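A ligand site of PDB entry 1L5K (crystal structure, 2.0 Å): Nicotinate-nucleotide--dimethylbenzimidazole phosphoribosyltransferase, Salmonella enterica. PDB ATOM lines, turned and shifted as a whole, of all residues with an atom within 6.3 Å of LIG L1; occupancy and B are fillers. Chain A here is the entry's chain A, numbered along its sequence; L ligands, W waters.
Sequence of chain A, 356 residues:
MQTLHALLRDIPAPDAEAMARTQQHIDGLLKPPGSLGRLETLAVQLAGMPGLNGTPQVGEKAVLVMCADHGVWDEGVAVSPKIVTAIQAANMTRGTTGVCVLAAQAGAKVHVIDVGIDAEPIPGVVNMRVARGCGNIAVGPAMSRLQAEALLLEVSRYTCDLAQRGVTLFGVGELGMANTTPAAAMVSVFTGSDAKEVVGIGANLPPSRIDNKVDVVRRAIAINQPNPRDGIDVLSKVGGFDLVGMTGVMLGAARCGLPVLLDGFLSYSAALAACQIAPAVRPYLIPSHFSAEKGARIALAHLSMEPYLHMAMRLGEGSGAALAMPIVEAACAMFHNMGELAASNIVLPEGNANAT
OG of Ser 291 sits at hydrogen-bond distance from O1 of LIG L1 (2.6 Å). An oxygen (O1) of LIG L1 sits at hydrogen-bond distance from the backbone NH of Phe 265 (2.9 Å). An oxygen (O2) of LG2 L2 is in hydrogen-bond range of the backbone NH (N) of Ala 203 (2.9 Å). The backbone NH (N) of Thr 180 lies within hydrogen-bond range of an oxygen (O1) of LG2 L2, at 3.1 Å. OG1 of Thr 180 is in hydrogen-bond range of O1 of LG2 L2, 2.6 Å away. The side-chain carboxylate of Glu 174 is in hydrogen-bond range of an oxygen (O7) of LG2 L2 (2.6 Å). A nitrogen (N1) of LG2 L2 sits at hydrogen-bond distance from the side-chain carboxylate (OE2) of Glu 317 (2.5 Å).
N of Glu 293 lies close to OG of Ser 291, at 3.1 Å. OH of Tyr 268 lies within hydrogen-bond range of N of Ser 291, 3.0 Å away. The guanidinium group of Arg 314 lies within hydrogen-bond range of the side-chain amide oxygen of Asn 204. O of Gly 264 lies within hydrogen-bond range of OG of Ser 267 (2.6 Å). The side-chain carboxylate (OE2) of Glu 293 lies within hydrogen-bond range of the backbone NH (N) of Gly 202, 3.2 Å away.
Merely in contact with LIG L1: Gly 316 (3.4 Å), Leu 266 (3.4 Å), Arg 314 (3.4 Å), Gly 264 (3.4 Å), Gly 202 (3.6 Å), Leu 315 (3.7 Å), Ala 203 (3.9 Å), Thr 180 (3.9 Å) and Glu 293 (3.97 Å).
Water W2 lies within hydrogen-bond range of O2 of LIG L1 (2.8 Å), OD2 of Asp 263 (2.9 Å), N of Gly 316 (3.2 Å), N of Gly 264 (3.4 Å) and NE2 of His 289 (3.4 Å). Water W1 lies within hydrogen-bond range of the side-chain carboxylate (OE2) of Glu 293 (2.8 Å) and the backbone carbonyl oxygen (O) of Gly 202 (3.0 Å).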
ATOM      1  N   GLU A 174     -12.513  10.963  24.421  1.00  0.00           N
ATOM      2  CA  GLU A 174     -13.146  11.108  23.115  1.00  0.00           C
ATOM      3  C   GLU A 174     -14.545  11.692  23.185  1.00  0.00           C
ATOM      4  O   GLU A 174     -15.112  11.859  24.274  1.00  0.00           O
ATOM      5  CB  GLU A 174     -13.205   9.744  22.407  1.00  0.00           C
ATOM      6  CG  GLU A 174     -13.647   8.591  23.314  1.00  0.00           C
ATOM      7  CD  GLU A 174     -14.962   8.865  24.013  1.00  0.00           C
ATOM      8  OE1 GLU A 174     -16.000   9.007  23.337  1.00  0.00           O
ATOM      9  OE2 GLU A 174     -14.955   8.939  25.260  1.00  0.00           O
ATOM     10  N   ASN A 179     -19.705   6.090  18.547  1.00  0.00           N
ATOM     11  CA  ASN A 179     -18.369   5.481  18.563  1.00  0.00           C
ATOM     12  C   ASN A 179     -18.192   4.190  19.346  1.00  0.00           C
ATOM     13  O   ASN A 179     -17.140   3.557  19.253  1.00  0.00           O
ATOM     14  CB  ASN A 179     -17.276   6.517  18.945  1.00  0.00           C
ATOM     15  CG  ASN A 179     -17.370   7.028  20.377  1.00  0.00           C
ATOM     16  OD1 ASN A 179     -18.223   6.621  21.157  1.00  0.00           O
ATOM     17  ND2 ASN A 179     -16.462   7.944  20.730  1.00  0.00           N
ATOM     18  N   THR A 180     -19.197   3.768  20.114  1.00  0.00           N
ATOM     19  CA  THR A 180     -19.046   2.506  20.834  1.00  0.00           C
ATOM     20  C   THR A 180     -19.256   1.320  19.873  1.00  0.00           C
ATOM     21  O   THR A 180     -18.961   0.176  20.212  1.00  0.00           O
ATOM     22  CB  THR A 180     -20.033   2.381  22.042  1.00  0.00           C
ATOM     23  OG1 THR A 180     -21.387   2.408  21.578  1.00  0.00           O
ATOM     24  CG2 THR A 180     -19.796   3.535  23.022  1.00  0.00           C
ATOM     25  N   ILE A 201     -24.714  -1.050  25.465  1.00  0.00           N
ATOM     26  CA  ILE A 201     -25.758  -0.039  25.278  1.00  0.00           C
ATOM     27  C   ILE A 201     -25.222   1.355  24.960  1.00  0.00           C
ATOM     28  O   ILE A 201     -25.996   2.271  24.651  1.00  0.00           O
ATOM     29  CB  ILE A 201     -26.652   0.022  26.538  1.00  0.00           C
ATOM     30  N   GLY A 202     -23.904   1.532  25.054  1.00  0.00           N
ATOM     31  CA  GLY A 202     -23.323   2.834  24.769  1.00  0.00           C
ATOM     32  C   GLY A 202     -24.030   3.935  25.547  1.00  0.00           C
ATOM     33  O   GLY A 202     -24.246   3.810  26.752  1.00  0.00           O
ATOM     34  N   ALA A 203     -24.394   5.014  24.867  1.00  0.00           N
ATOM     35  CA  ALA A 203     -25.080   6.117  25.518  1.00  0.00           C
ATOM     36  C   ALA A 203     -26.592   5.875  25.551  1.00  0.00           C
ATOM     37  O   ALA A 203     -27.355   6.446  24.770  1.00  0.00           O
ATOM     38  CB  ALA A 203     -24.777   7.434  24.787  1.00  0.00           C
ATOM     39  N   ASN A 204     -27.010   4.998  26.467  1.00  0.00           N
ATOM     40  CA  ASN A 204     -28.413   4.645  26.665  1.00  0.00           C
ATOM     41  C   ASN A 204     -29.170   4.132  25.431  1.00  0.00           C
ATOM     42  O   ASN A 204     -30.277   4.594  25.155  1.00  0.00           O
ATOM     43  CB  ASN A 204     -29.186   5.824  27.270  1.00  0.00           C
ATOM     44  CG  ASN A 204     -28.712   6.180  28.657  1.00  0.00           C
ATOM     45  OD1 ASN A 204     -28.409   5.300  29.473  1.00  0.00           O
ATOM     46  ND2 ASN A 204     -28.639   7.476  28.950  1.00  0.00           N
ATOM     47  N   ASP A 263      -9.176   5.766  29.848  1.00  0.00           N
ATOM     48  CA  ASP A 263     -10.465   6.199  30.342  1.00  0.00           C
ATOM     49  C   ASP A 263     -11.379   4.992  30.386  1.00  0.00           C
ATOM     50  O   ASP A 263     -11.161   4.077  31.192  1.00  0.00           O
ATOM     51  CB  ASP A 263     -11.052   7.298  29.420  1.00  0.00           C
ATOM     52  CG  ASP A 263     -12.373   7.866  29.928  1.00  0.00           C
ATOM     53  OD1 ASP A 263     -12.595   7.896  31.160  1.00  0.00           O
ATOM     54  OD2 ASP A 263     -13.190   8.302  29.098  1.00  0.00           O
ATOM     55  N   GLY A 264     -12.394   4.976  29.526  1.00  0.00           N
ATOM     56  CA  GLY A 264     -13.321   3.860  29.482  1.00  0.00           C
ATOM     57  C   GLY A 264     -13.215   2.955  28.265  1.00  0.00           C
ATOM     58  O   GLY A 264     -12.141   2.824  27.667  1.00  0.00           O
ATOM     59  N   PHE A 265     -14.339   2.325  27.912  1.00  0.00           N
ATOM     60  CA  PHE A 265     -14.415   1.388  26.785  1.00  0.00           C
ATOM     61  C   PHE A 265     -13.802   1.852  25.473  1.00  0.00           C
ATOM     62  O   PHE A 265     -13.117   1.079  24.807  1.00  0.00           O
ATOM     63  CB  PHE A 265     -15.880   0.982  26.544  1.00  0.00           C
ATOM     64  CG  PHE A 265     -16.035  -0.191  25.596  1.00  0.00           C
ATOM     65  CD1 PHE A 265     -16.640  -0.020  24.346  1.00  0.00           C
ATOM     66  CD2 PHE A 265     -15.576  -1.450  25.952  1.00  0.00           C
ATOM     67  CE1 PHE A 265     -16.767  -1.096  23.469  1.00  0.00           C
ATOM     68  CE2 PHE A 265     -15.706  -2.535  25.074  1.00  0.00           C
ATOM     69  CZ  PHE A 265     -16.301  -2.358  23.833  1.00  0.00           C
ATOM     70  N   LEU A 266     -14.041   3.102  25.088  1.00  0.00           N
ATOM     71  CA  LEU A 266     -13.457   3.597  23.842  1.00  0.00           C
ATOM     72  C   LEU A 266     -11.935   3.574  23.940  1.00  0.00           C
ATOM     73  O   LEU A 266     -11.249   3.181  22.987  1.00  0.00           O
ATOM     74  CB  LEU A 266     -13.924   5.031  23.536  1.00  0.00           C
ATOM     75  CG  LEU A 266     -15.407   5.278  23.206  1.00  0.00           C
ATOM     76  CD1 LEU A 266     -15.890   4.257  22.190  1.00  0.00           C
ATOM     77  CD2 LEU A 266     -16.248   5.197  24.459  1.00  0.00           C
ATOM     78  N   SER A 267     -11.398   3.966  25.093  1.00  0.00           N
ATOM     79  CA  SER A 267      -9.954   3.986  25.276  1.00  0.00           C
ATOM     80  C   SER A 267      -9.367   2.576  25.251  1.00  0.00           C
ATOM     81  O   SER A 267      -8.246   2.370  24.775  1.00  0.00           O
ATOM     82  CB  SER A 267      -9.575   4.698  26.588  1.00  0.00           C
ATOM     83  OG  SER A 267      -9.774   3.880  27.727  1.00  0.00           O
ATOM     84  N   TYR A 268     -10.118   1.607  25.766  1.00  0.00           N
ATOM     85  CA  TYR A 268      -9.661   0.210  25.776  1.00  0.00           C
ATOM     86  C   TYR A 268      -9.425  -0.270  24.345  1.00  0.00           C
ATOM     87  O   TYR A 268      -8.441  -0.949  24.069  1.00  0.00           O
ATOM     88  CB  TYR A 268     -10.687  -0.723  26.405  1.00  0.00           C
ATOM     89  CG  TYR A 268     -11.113  -0.449  27.833  1.00  0.00           C
ATOM     90  CD1 TYR A 268     -12.263  -1.031  28.341  1.00  0.00           C
ATOM     91  CD2 TYR A 268     -10.396   0.422  28.667  1.00  0.00           C
ATOM     92  CE1 TYR A 268     -12.729  -0.755  29.623  1.00  0.00           C
ATOM     93  CE2 TYR A 268     -10.853   0.703  29.972  1.00  0.00           C
ATOM     94  CZ  TYR A 268     -12.026   0.115  30.428  1.00  0.00           C
ATOM     95  OH  TYR A 268     -12.546   0.425  31.660  1.00  0.00           O
ATOM     96  N   HIS A 289     -10.652   3.546  35.526  1.00  0.00           N
ATOM     97  CA  HIS A 289     -11.843   2.907  36.074  1.00  0.00           C
ATOM     98  C   HIS A 289     -12.293   1.724  35.226  1.00  0.00           C
ATOM     99  O   HIS A 289     -11.757   1.481  34.146  1.00  0.00           O
ATOM    100  CB  HIS A 289     -12.993   3.917  36.173  1.00  0.00           C
ATOM    101  CG  HIS A 289     -13.589   4.275  34.855  1.00  0.00           C
ATOM    102  ND1 HIS A 289     -12.880   4.916  33.865  1.00  0.00           N
ATOM    103  CD2 HIS A 289     -14.832   4.084  34.357  1.00  0.00           C
ATOM    104  CE1 HIS A 289     -13.654   5.108  32.813  1.00  0.00           C
ATOM    105  NE2 HIS A 289     -14.857   4.620  33.087  1.00  0.00           N
ATOM    106  N   SER A 291     -15.161   0.445  33.093  1.00  0.00           N
ATOM    107  CA  SER A 291     -16.356   0.865  32.363  1.00  0.00           C
ATOM    108  C   SER A 291     -17.552  -0.070  32.501  1.00  0.00           C
ATOM    109  O   SER A 291     -17.397  -1.293  32.526  1.00  0.00           O
ATOM    110  CB  SER A 291     -16.034   1.013  30.868  1.00  0.00           C
ATOM    111  OG  SER A 291     -17.208   1.311  30.137  1.00  0.00           O
ATOM    112  N   ALA A 292     -18.750   0.517  32.563  1.00  0.00           N
ATOM    113  CA  ALA A 292     -19.985  -0.258  32.705  1.00  0.00           C
ATOM    114  C   ALA A 292     -20.434  -0.840  31.369  1.00  0.00           C
ATOM    115  O   ALA A 292     -21.497  -1.463  31.271  1.00  0.00           O
ATOM    116  CB  ALA A 292     -21.092   0.627  33.269  1.00  0.00           C
ATOM    117  N   GLU A 293     -19.641  -0.628  30.323  1.00  0.00           N
ATOM    118  CA  GLU A 293     -19.966  -1.166  29.009  1.00  0.00           C
ATOM    119  C   GLU A 293     -19.780  -2.692  29.090  1.00  0.00           C
ATOM    120  O   GLU A 293     -18.854  -3.176  29.736  1.00  0.00           O
ATOM    121  CB  GLU A 293     -19.022  -0.538  27.977  1.00  0.00           C
ATOM    122  CG  GLU A 293     -19.225  -0.957  26.537  1.00  0.00           C
ATOM    123  CD  GLU A 293     -20.389  -0.266  25.836  1.00  0.00           C
ATOM    124  OE1 GLU A 293     -20.433  -0.340  24.594  1.00  0.00           O
ATOM    125  OE2 GLU A 293     -21.265   0.322  26.507  1.00  0.00           O
ATOM    126  N   MET A 313     -19.085   3.828  35.738  1.00  0.00           N
ATOM    127  CA  MET A 313     -19.153   4.955  34.835  1.00  0.00           C
ATOM    128  C   MET A 313     -19.187   4.555  33.352  1.00  0.00           C
ATOM    129  O   MET A 313     -18.652   3.512  32.955  1.00  0.00           O
ATOM    130  CB  MET A 313     -17.997   5.923  35.120  1.00  0.00           C
ATOM    131  CG  MET A 313     -18.248   6.773  36.369  1.00  0.00           C
ATOM    132  SD  MET A 313     -16.790   7.649  37.007  1.00  0.00           S
ATOM    133  CE  MET A 313     -16.331   8.661  35.597  1.00  0.00           C
ATOM    134  N   ARG A 314     -19.854   5.384  32.554  1.00  0.00           N
ATOM    135  CA  ARG A 314     -19.997   5.136  31.118  1.00  0.00           C
ATOM    136  C   ARG A 314     -20.298   6.437  30.378  1.00  0.00           C
ATOM    137  O   ARG A 314     -21.189   6.488  29.521  1.00  0.00           O
ATOM    138  CB  ARG A 314     -21.125   4.120  30.886  1.00  0.00           C
ATOM    139  CG  ARG A 314     -22.444   4.450  31.572  1.00  0.00           C
ATOM    140  CD  ARG A 314     -23.477   3.337  31.370  1.00  0.00           C
ATOM    141  NE  ARG A 314     -24.693   3.527  32.144  1.00  0.00           N
ATOM    142  CZ  ARG A 314     -25.711   4.320  31.803  1.00  0.00           C
ATOM    143  NH1 ARG A 314     -25.668   5.016  30.666  1.00  0.00           N
ATOM    144  NH2 ARG A 314     -26.774   4.410  32.583  1.00  0.00           N
ATOM    145  N   LEU A 315     -19.561   7.493  30.716  1.00  0.00           N
ATOM    146  CA  LEU A 315     -19.748   8.787  30.069  1.00  0.00           C
ATOM    147  C   LEU A 315     -18.707   9.004  28.977  1.00  0.00           C
ATOM    148  O   LEU A 315     -19.019   9.543  27.916  1.00  0.00           O
ATOM    149  CB  LEU A 315     -19.634   9.931  31.082  1.00  0.00           C
ATOM    150  CG  LEU A 315     -19.526  11.349  30.493  1.00  0.00           C
ATOM    151  CD1 LEU A 315     -20.792  11.702  29.713  1.00  0.00           C
ATOM    152  CD2 LEU A 315     -19.309  12.359  31.624  1.00  0.00           C
ATOM    153  N   GLY A 316     -17.473   8.591  29.232  1.00  0.00           N
ATOM    154  CA  GLY A 316     -16.427   8.811  28.248  1.00  0.00           C
ATOM    155  C   GLY A 316     -15.874  10.216  28.461  1.00  0.00           C
ATOM    156  O   GLY A 316     -15.885  10.727  29.584  1.00  0.00           O
ATOM    157  N   GLU A 317     -15.418  10.842  27.380  1.00  0.00           N
ATOM    158  CA  GLU A 317     -14.853  12.197  27.409  1.00  0.00           C
ATOM    159  C   GLU A 317     -13.497  12.271  28.107  1.00  0.00           C
ATOM    160  O   GLU A 317     -12.821  13.306  28.074  1.00  0.00           O
ATOM    161  CB  GLU A 317     -15.799  13.183  28.098  1.00  0.00           C
ATOM    162  CG  GLU A 317     -17.195  13.277  27.489  1.00  0.00           C
ATOM    163  CD  GLU A 317     -18.033  14.390  28.095  1.00  0.00           C
ATOM    164  OE1 GLU A 317     -17.520  15.130  28.955  1.00  0.00           O
ATOM    165  OE2 GLU A 317     -19.217  14.521  27.721  1.00  0.00           O
HETATM  166  N1  LIG L   1     -19.757   6.238  26.245  1.00  0.00           N
HETATM  167  C1  LIG L   1     -18.509   6.070  26.812  1.00  0.00           C
HETATM  168  C2  LIG L   1     -18.286   4.877  27.554  1.00  0.00           C
HETATM  169  C3  LIG L   1     -19.341   3.873  27.722  1.00  0.00           C
HETATM  170  C4  LIG L   1     -20.565   4.183  27.082  1.00  0.00           C
HETATM  171  C5  LIG L   1     -20.848   5.330  26.345  1.00  0.00           C
HETATM  172  C6  LIG L   1     -16.914   4.637  28.206  1.00  0.00           C
HETATM  173  O1  LIG L   1     -16.720   3.581  28.863  1.00  0.00           O
HETATM  174  O2  LIG L   1     -15.981   5.491  28.081  1.00  0.00           O
HETATM  175  N1  LG2 L   2     -20.432  12.750  26.364  1.00  0.00           N
HETATM  176  N2  LG2 L   2     -20.718  10.693  25.386  1.00  0.00           N
HETATM  177  C1  LG2 L   2     -19.925  11.536  26.115  1.00  0.00           C
HETATM  178  C2  LG2 L   2     -21.865  11.511  25.138  1.00  0.00           C
HETATM  179  C3  LG2 L   2     -21.660  12.791  25.768  1.00  0.00           C
HETATM  180  C4  LG2 L   2     -22.657  13.822  25.701  1.00  0.00           C
HETATM  181  C5  LG2 L   2     -23.846  13.569  25.006  1.00  0.00           C
HETATM  182  C6  LG2 L   2     -24.074  12.288  24.367  1.00  0.00           C
HETATM  183  C7  LG2 L   2     -23.096  11.264  24.426  1.00  0.00           C
HETATM  184  P1  LG2 L   2     -22.919   5.717  21.560  1.00  0.00           P
HETATM  185  O1  LG2 L   2     -22.106   4.746  20.756  1.00  0.00           O
HETATM  186  O2  LG2 L   2     -24.190   5.075  22.009  1.00  0.00           O
HETATM  187  O3  LG2 L   2     -23.236   6.911  20.719  1.00  0.00           O
HETATM  188  O4  LG2 L   2     -22.081   6.188  22.844  1.00  0.00           O
HETATM  189  C8  LG2 L   2     -20.815   6.820  22.686  1.00  0.00           C
HETATM  190  C9  LG2 L   2     -21.010   8.337  22.818  1.00  0.00           C
HETATM  191  O5  LG2 L   2     -21.490   8.715  24.155  1.00  0.00           O
HETATM  192  C10 LG2 L   2     -19.744   9.160  22.656  1.00  0.00           C
HETATM  193  O6  LG2 L   2     -20.022  10.521  22.239  1.00  0.00           O
HETATM  194  C11 LG2 L   2     -19.199   9.100  24.059  1.00  0.00           C
HETATM  195  O7  LG2 L   2     -18.192  10.100  24.223  1.00  0.00           O
HETATM  196  C12 LG2 L   2     -20.422   9.256  24.936  1.00  0.00           C
HETATM  197  O   HOH W   1     -22.733   1.770  28.341  1.00  0.00           O
HETATM  198  O   HOH W   2     -15.134   6.696  30.440  1.00  0.00           O
HETATM  199  O   HOH W   3     -13.547   5.558  26.926  1.00  0.00           O
